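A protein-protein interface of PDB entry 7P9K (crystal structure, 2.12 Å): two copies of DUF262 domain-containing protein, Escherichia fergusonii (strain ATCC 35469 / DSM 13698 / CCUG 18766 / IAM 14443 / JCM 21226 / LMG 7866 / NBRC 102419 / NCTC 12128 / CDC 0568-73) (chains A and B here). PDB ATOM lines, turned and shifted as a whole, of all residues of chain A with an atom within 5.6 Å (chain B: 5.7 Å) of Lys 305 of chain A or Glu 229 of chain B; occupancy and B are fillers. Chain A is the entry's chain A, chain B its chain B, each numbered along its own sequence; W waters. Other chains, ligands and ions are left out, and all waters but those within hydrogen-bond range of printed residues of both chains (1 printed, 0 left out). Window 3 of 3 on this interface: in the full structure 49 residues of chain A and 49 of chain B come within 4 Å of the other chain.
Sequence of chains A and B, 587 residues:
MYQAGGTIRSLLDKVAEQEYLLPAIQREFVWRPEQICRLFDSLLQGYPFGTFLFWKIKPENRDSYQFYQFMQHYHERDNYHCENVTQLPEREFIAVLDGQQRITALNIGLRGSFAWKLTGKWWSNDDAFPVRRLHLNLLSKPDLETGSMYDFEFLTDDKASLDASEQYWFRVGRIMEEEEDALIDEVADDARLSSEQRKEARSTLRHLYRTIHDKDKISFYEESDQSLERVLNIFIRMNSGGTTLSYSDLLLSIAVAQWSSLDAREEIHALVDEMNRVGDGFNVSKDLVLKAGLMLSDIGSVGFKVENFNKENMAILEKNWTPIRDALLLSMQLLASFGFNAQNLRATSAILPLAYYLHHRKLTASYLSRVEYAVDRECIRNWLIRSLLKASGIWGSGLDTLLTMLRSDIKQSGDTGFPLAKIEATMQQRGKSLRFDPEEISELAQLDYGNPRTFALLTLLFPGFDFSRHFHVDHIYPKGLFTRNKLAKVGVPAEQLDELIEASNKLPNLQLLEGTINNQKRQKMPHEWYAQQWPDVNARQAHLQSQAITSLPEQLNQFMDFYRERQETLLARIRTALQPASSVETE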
ATOM      1  N   TYR A 247      12.095  -2.621  -0.045  1.00  0.00           N
ATOM      2  CA  TYR A 247      12.908  -2.464  -1.253  1.00  0.00           C
ATOM      3  C   TYR A 247      12.099  -2.790  -2.506  1.00  0.00           C
ATOM      4  O   TYR A 247      12.177  -2.072  -3.512  1.00  0.00           O
ATOM      5  CB  TYR A 247      14.160  -3.345  -1.166  1.00  0.00           C
ATOM      6  CG  TYR A 247      15.219  -3.091  -2.232  1.00  0.00           C
ATOM      7  CD1 TYR A 247      16.029  -1.963  -2.186  1.00  0.00           C
ATOM      8  CD2 TYR A 247      15.426  -4.002  -3.276  1.00  0.00           C
ATOM      9  CE1 TYR A 247      17.015  -1.738  -3.151  1.00  0.00           C
ATOM     10  CE2 TYR A 247      16.410  -3.785  -4.241  1.00  0.00           C
ATOM     11  CZ  TYR A 247      17.197  -2.649  -4.179  1.00  0.00           C
ATOM     12  OH  TYR A 247      18.167  -2.422  -5.147  1.00  0.00           O
ATOM     13  N   LEU A 251      11.244  -0.403  -5.740  1.00  0.00           N
ATOM     14  CA  LEU A 251      11.517  -0.681  -7.146  1.00  0.00           C
ATOM     15  C   LEU A 251      10.264  -0.509  -7.997  1.00  0.00           C
ATOM     16  O   LEU A 251      10.308   0.098  -9.075  1.00  0.00           O
ATOM     17  CB  LEU A 251      12.088  -2.090  -7.298  1.00  0.00           C
ATOM     18  CG  LEU A 251      13.605  -2.179  -7.404  1.00  0.00           C
ATOM     19  CD1 LEU A 251      14.276  -1.255  -6.378  1.00  0.00           C
ATOM     20  CD2 LEU A 251      14.039  -3.614  -7.219  1.00  0.00           C
ATOM     21  N   LEU A 294      12.989  -7.302 -17.101  1.00  0.00           N
ATOM     22  CA  LEU A 294      14.409  -7.088 -17.376  1.00  0.00           C
ATOM     23  C   LEU A 294      14.964  -8.175 -18.289  1.00  0.00           C
ATOM     24  O   LEU A 294      15.713  -7.881 -19.237  1.00  0.00           O
ATOM     25  CB  LEU A 294      15.204  -7.011 -16.076  1.00  0.00           C
ATOM     26  CG  LEU A 294      14.848  -5.847 -15.127  1.00  0.00           C
ATOM     27  CD1 LEU A 294      15.755  -5.895 -13.892  1.00  0.00           C
ATOM     28  CD2 LEU A 294      14.940  -4.465 -15.812  1.00  0.00           C
ATOM     29  N   GLY A 303      19.358  -8.541 -12.299  1.00  0.00           N
ATOM     30  CA  GLY A 303      19.300  -8.310 -10.877  1.00  0.00           C
ATOM     31  C   GLY A 303      18.101  -7.474 -10.498  1.00  0.00           C
ATOM     32  O   GLY A 303      17.817  -6.448 -11.121  1.00  0.00           O
ATOM     33  N   PHE A 304      17.374  -7.921  -9.477  1.00  0.00           N
ATOM     34  CA  PHE A 304      16.259  -7.154  -8.942  1.00  0.00           C
ATOM     35  C   PHE A 304      16.798  -6.020  -8.068  1.00  0.00           C
ATOM     36  O   PHE A 304      16.544  -5.941  -6.871  1.00  0.00           O
ATOM     37  CB  PHE A 304      15.326  -8.072  -8.165  1.00  0.00           C
ATOM     38  CG  PHE A 304      14.012  -7.459  -7.849  1.00  0.00           C
ATOM     39  CD1 PHE A 304      13.162  -7.055  -8.874  1.00  0.00           C
ATOM     40  CD2 PHE A 304      13.613  -7.281  -6.527  1.00  0.00           C
ATOM     41  CE1 PHE A 304      11.934  -6.476  -8.587  1.00  0.00           C
ATOM     42  CE2 PHE A 304      12.386  -6.707  -6.230  1.00  0.00           C
ATOM     43  CZ  PHE A 304      11.543  -6.303  -7.265  1.00  0.00           C
ATOM     44  N   LYS A 305      17.577  -5.141  -8.700  1.00  0.00           N
ATOM     45  CA  LYS A 305      18.261  -4.043  -8.030  1.00  0.00           C
ATOM     46  C   LYS A 305      17.768  -2.713  -8.592  1.00  0.00           C
ATOM     47  O   LYS A 305      17.489  -2.597  -9.793  1.00  0.00           O
ATOM     48  CB  LYS A 305      19.781  -4.147  -8.208  1.00  0.00           C
ATOM     49  CG  LYS A 305      20.409  -5.409  -7.607  1.00  0.00           C
ATOM     50  CD  LYS A 305      21.122  -5.110  -6.283  1.00  0.00           C
ATOM     51  CE  LYS A 305      20.741  -6.106  -5.180  1.00  0.00           C
ATOM     52  NZ  LYS A 305      21.093  -5.556  -3.828  1.00  0.00           N
ATOM     53  N   VAL A 306      17.681  -1.700  -7.715  1.00  0.00           N
ATOM     54  CA  VAL A 306      17.165  -0.384  -8.118  1.00  0.00           C
ATOM     55  C   VAL A 306      17.977   0.192  -9.275  1.00  0.00           C
ATOM     56  O   VAL A 306      17.426   0.868 -10.154  1.00  0.00           O
ATOM     57  CB  VAL A 306      17.150   0.591  -6.916  1.00  0.00           C
ATOM     58  CG1 VAL A 306      18.515   1.270  -6.722  1.00  0.00           C
ATOM     59  CG2 VAL A 306      16.055   1.629  -7.069  1.00  0.00           C
ATOM     60  N   GLU A 307      19.287  -0.080  -9.320  1.00  0.00           N
ATOM     61  CA  GLU A 307      20.111   0.474 -10.391  1.00  0.00           C
ATOM     62  C   GLU A 307      19.660   0.006 -11.767  1.00  0.00           C
ATOM     63  O   GLU A 307      19.962   0.669 -12.761  1.00  0.00           O
ATOM     64  CB  GLU A 307      21.574   0.106 -10.191  1.00  0.00           C
ATOM     65  CG  GLU A 307      21.801  -1.330  -9.746  1.00  0.00           C
ATOM     66  CD  GLU A 307      22.054  -1.468  -8.226  1.00  0.00           C
ATOM     67  OE1 GLU A 307      21.140  -1.144  -7.409  1.00  0.00           O
ATOM     68  OE2 GLU A 307      23.171  -1.919  -7.858  1.00  0.00           O
ATOM     69  N   ASN A 308      18.966  -1.123 -11.861  1.00  0.00           N
ATOM     70  CA  ASN A 308      18.520  -1.605 -13.160  1.00  0.00           C
ATOM     71  C   ASN A 308      17.217  -0.977 -13.594  1.00  0.00           C
ATOM     72  O   ASN A 308      16.718  -1.319 -14.676  1.00  0.00           O
ATOM     73  CB  ASN A 308      18.347  -3.123 -13.147  1.00  0.00           C
ATOM     74  CG  ASN A 308      19.653  -3.839 -13.078  1.00  0.00           C
ATOM     75  OD1 ASN A 308      20.670  -3.322 -13.532  1.00  0.00           O
ATOM     76  ND2 ASN A 308      19.650  -5.029 -12.497  1.00  0.00           N
ATOM     77  N   PHE A 309      16.637  -0.105 -12.773  1.00  0.00           N
ATOM     78  CA  PHE A 309      15.365   0.520 -13.108  1.00  0.00           C
ATOM     79  C   PHE A 309      15.523   2.021 -13.352  1.00  0.00           C
ATOM     80  O   PHE A 309      14.615   2.804 -13.079  1.00  0.00           O
ATOM     81  CB  PHE A 309      14.330   0.208 -12.029  1.00  0.00           C
ATOM     82  CG  PHE A 309      13.983  -1.252 -11.959  1.00  0.00           C
ATOM     83  CD1 PHE A 309      14.790  -2.134 -11.258  1.00  0.00           C
ATOM     84  CD2 PHE A 309      12.889  -1.754 -12.641  1.00  0.00           C
ATOM     85  CE1 PHE A 309      14.506  -3.490 -11.216  1.00  0.00           C
ATOM     86  CE2 PHE A 309      12.592  -3.106 -12.610  1.00  0.00           C
ATOM     87  CZ  PHE A 309      13.404  -3.979 -11.887  1.00  0.00           C
ATOM     88  N   SER B 224      24.195   4.198  -0.551  1.00  0.00           N
ATOM     89  CA  SER B 224      24.273   4.213  -2.006  1.00  0.00           C
ATOM     90  C   SER B 224      23.444   3.091  -2.623  1.00  0.00           C
ATOM     91  O   SER B 224      22.869   2.250  -1.929  1.00  0.00           O
ATOM     92  CB  SER B 224      25.713   4.036  -2.453  1.00  0.00           C
ATOM     93  OG  SER B 224      26.060   2.666  -2.278  1.00  0.00           O
ATOM     94  N   ASP B 225      23.433   3.061  -3.963  1.00  0.00           N
ATOM     95  CA  ASP B 225      22.709   2.033  -4.712  1.00  0.00           C
ATOM     96  C   ASP B 225      23.113   0.634  -4.273  1.00  0.00           C
ATOM     97  O   ASP B 225      22.279  -0.277  -4.234  1.00  0.00           O
ATOM     98  CB  ASP B 225      22.974   2.172  -6.218  1.00  0.00           C
ATOM     99  CG  ASP B 225      22.134   3.255  -6.871  1.00  0.00           C
ATOM    100  OD1 ASP B 225      21.421   3.979  -6.137  1.00  0.00           O
ATOM    101  OD2 ASP B 225      22.196   3.392  -8.124  1.00  0.00           O
ATOM    102  N   GLN B 226      24.397   0.439  -3.964  1.00  0.00           N
ATOM    103  CA  GLN B 226      24.919  -0.919  -3.915  1.00  0.00           C
ATOM    104  C   GLN B 226      24.409  -1.653  -2.691  1.00  0.00           C
ATOM    105  O   GLN B 226      24.020  -2.825  -2.779  1.00  0.00           O
ATOM    106  CB  GLN B 226      26.448  -0.918  -3.959  1.00  0.00           C
ATOM    107  CG  GLN B 226      27.018  -1.381  -5.313  1.00  0.00           C
ATOM    108  CD  GLN B 226      27.172  -2.904  -5.424  1.00  0.00           C
ATOM    109  OE1 GLN B 226      27.257  -3.604  -4.411  1.00  0.00           O
ATOM    110  NE2 GLN B 226      27.193  -3.421  -6.659  1.00  0.00           N
ATOM    111  N   SER B 227      24.373  -0.975  -1.549  1.00  0.00           N
ATOM    112  CA  SER B 227      23.914  -1.591  -0.319  1.00  0.00           C
ATOM    113  C   SER B 227      22.613  -0.977   0.194  1.00  0.00           C
ATOM    114  O   SER B 227      22.261  -1.165   1.363  1.00  0.00           O
ATOM    115  CB  SER B 227      25.020  -1.513   0.725  1.00  0.00           C
ATOM    116  OG  SER B 227      26.082  -2.386   0.354  1.00  0.00           O
ATOM    117  N   LEU B 228      21.881  -0.263  -0.665  1.00  0.00           N
ATOM    118  CA  LEU B 228      20.563   0.222  -0.272  1.00  0.00           C
ATOM    119  C   LEU B 228      19.700  -0.929   0.233  1.00  0.00           C
ATOM    120  O   LEU B 228      19.059  -0.830   1.282  1.00  0.00           O
ATOM    121  CB  LEU B 228      19.885   0.946  -1.448  1.00  0.00           C
ATOM    122  CG  LEU B 228      18.516   1.596  -1.179  1.00  0.00           C
ATOM    123  CD1 LEU B 228      18.602   2.719  -0.143  1.00  0.00           C
ATOM    124  CD2 LEU B 228      17.894   2.126  -2.455  1.00  0.00           C
ATOM    125  N   GLU B 229      19.681  -2.041  -0.505  1.00  0.00           N
ATOM    126  CA  GLU B 229      18.743  -3.114  -0.199  1.00  0.00           C
ATOM    127  C   GLU B 229      18.969  -3.651   1.198  1.00  0.00           C
ATOM    128  O   GLU B 229      18.014  -3.912   1.932  1.00  0.00           O
ATOM    129  CB  GLU B 229      18.886  -4.241  -1.205  1.00  0.00           C
ATOM    130  CG  GLU B 229      18.367  -5.563  -0.693  1.00  0.00           C
ATOM    131  CD  GLU B 229      17.809  -6.454  -1.803  1.00  0.00           C
ATOM    132  OE1 GLU B 229      16.625  -6.862  -1.703  1.00  0.00           O
ATOM    133  OE2 GLU B 229      18.560  -6.733  -2.770  1.00  0.00           O
ATOM    134  N   ARG B 230      20.231  -3.813   1.580  1.00  0.00           N
ATOM    135  CA  ARG B 230      20.553  -4.404   2.867  1.00  0.00           C
ATOM    136  C   ARG B 230      20.184  -3.464   4.011  1.00  0.00           C
ATOM    137  O   ARG B 230      19.519  -3.869   4.971  1.00  0.00           O
ATOM    138  CB  ARG B 230      22.037  -4.762   2.897  1.00  0.00           C
ATOM    139  CG  ARG B 230      22.548  -5.209   4.247  1.00  0.00           C
ATOM    140  CD  ARG B 230      24.037  -5.526   4.190  1.00  0.00           C
ATOM    141  NE  ARG B 230      24.856  -4.409   3.722  1.00  0.00           N
ATOM    142  CZ  ARG B 230      25.342  -3.448   4.513  1.00  0.00           C
ATOM    143  NH1 ARG B 230      25.077  -3.459   5.808  1.00  0.00           N
ATOM    144  NH2 ARG B 230      26.091  -2.469   4.013  1.00  0.00           N
ATOM    145  N   VAL B 231      20.580  -2.192   3.910  1.00  0.00           N
ATOM    146  CA  VAL B 231      20.355  -1.257   5.009  1.00  0.00           C
ATOM    147  C   VAL B 231      18.886  -0.871   5.096  1.00  0.00           C
ATOM    148  O   VAL B 231      18.348  -0.675   6.189  1.00  0.00           O
ATOM    149  CB  VAL B 231      21.260  -0.027   4.856  1.00  0.00           C
ATOM    150  CG1 VAL B 231      20.977   0.992   5.951  1.00  0.00           C
ATOM    151  CG2 VAL B 231      22.725  -0.456   4.875  1.00  0.00           C
ATOM    152  N   LEU B 232      18.206  -0.750   3.957  1.00  0.00           N
ATOM    153  CA  LEU B 232      16.771  -0.511   4.013  1.00  0.00           C
ATOM    154  C   LEU B 232      16.076  -1.602   4.824  1.00  0.00           C
ATOM    155  O   LEU B 232      15.221  -1.310   5.669  1.00  0.00           O
ATOM    156  CB  LEU B 232      16.194  -0.422   2.603  1.00  0.00           C
ATOM    157  CG  LEU B 232      14.685  -0.198   2.605  1.00  0.00           C
ATOM    158  CD1 LEU B 232      14.219   0.602   1.400  1.00  0.00           C
ATOM    159  CD2 LEU B 232      14.007  -1.555   2.610  1.00  0.00           C
ATOM    160  N   ASN B 233      16.441  -2.868   4.590  1.00  0.00           N
ATOM    161  CA  ASN B 233      15.904  -3.963   5.402  1.00  0.00           C
ATOM    162  C   ASN B 233      16.300  -3.817   6.881  1.00  0.00           C
ATOM    163  O   ASN B 233      15.452  -3.901   7.769  1.00  0.00           O
ATOM    164  CB  ASN B 233      16.360  -5.310   4.830  1.00  0.00           C
ATOM    165  CG  ASN B 233      15.677  -5.647   3.492  1.00  0.00           C
ATOM    166  OD1 ASN B 233      14.652  -5.052   3.138  1.00  0.00           O
ATOM    167  ND2 ASN B 233      16.251  -6.597   2.741  1.00  0.00           N
ATOM    168  N   ILE B 234      17.584  -3.604   7.171  1.00  0.00           N
ATOM    169  CA  ILE B 234      17.981  -3.321   8.554  1.00  0.00           C
ATOM    170  C   ILE B 234      17.110  -2.217   9.146  1.00  0.00           C
ATOM    171  O   ILE B 234      16.548  -2.360  10.235  1.00  0.00           O
ATOM    172  CB  ILE B 234      19.471  -2.947   8.633  1.00  0.00           C
ATOM    173  CG1 ILE B 234      20.341  -4.155   8.275  1.00  0.00           C
ATOM    174  CG2 ILE B 234      19.801  -2.436  10.042  1.00  0.00           C
ATOM    175  CD1 ILE B 234      21.817  -3.847   8.251  1.00  0.00           C
HETATM  176  O   HOH W   1      12.608  -4.468   1.739  1.00  0.00           O
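Tyr 247 of chain A touches Glu 229 of chain B (CD2 to OE1, 3.5 Å). N of Tyr 247 of chain A touches CD2 of Leu 232 of chain B, at 3.4 Å.
NZ of Lys 305 of chain A is in salt-bridge range of OE2 of Glu 229 of chain B (3.0 Å). The side-chain carboxylate (OE1) of Glu 307 of chain A sits close to the backbone carbonyl oxygen (O) of Asp 225 of chain B.
No position is printed for both chains.
Glu 229 of chain B touches just these residues of chain A: Tyr 247 and Lys 305. Of the printed residues of chain B, Glu 307 of chain A touches Asp 225 (3.5 Å). Of the printed residues of chain A, Asp 225 of chain B touches Glu 307 (3.5 Å). Of the printed residues of chain A, Leu 232 of chain B touches Tyr 247 (3.4 Å). The nearest residue of chain B that does not touch Lys 305 of chain A is Gln 226 of chain B (4.1 Å). The nearest residue of chain A that does not touch Glu 229 of chain B is Phe 304 of chain A (4.6 Å).
The backbone carbonyl oxygen (O) of Glu 229 of chain B lies close to the side-chain amide nitrogen (ND2) of Asn 233 of chain B. The backbone NH (N) of Val 306 of chain A lies within hydrogen-bond range of the side-chain hydroxyl (OH) of Tyr 247 of chain A, 2.7 Å away.
Of the 11 printed residues of chain B, 3 touch a printed residue of chain A. Printed residues of chain B that touch a printed residue of chain A: Asp 225, Glu 229 and Leu 232. Hydrophobic or aromatic side chains of chain B within 4 Å of the printed part of chain A: Leu 232. Hydrophobic or aromatic side chains of chain A that line the printed part of chain B: Tyr 247. Along chain A the printed residues that touch a printed residue of chain B span positions 247 to 307. Among the printed residues, 4 pairs touch across the chains. Among the printed residues, Asp or Glu carboxylates within 4 Å of a Lys or Arg side-chain nitrogen of the other chain: Lys 305 of chain A with Glu 229 of chain B (3.0 Å).
Water W1 bridges OD1 of Asn 233 of chain B and N of Tyr 247 of chain A.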
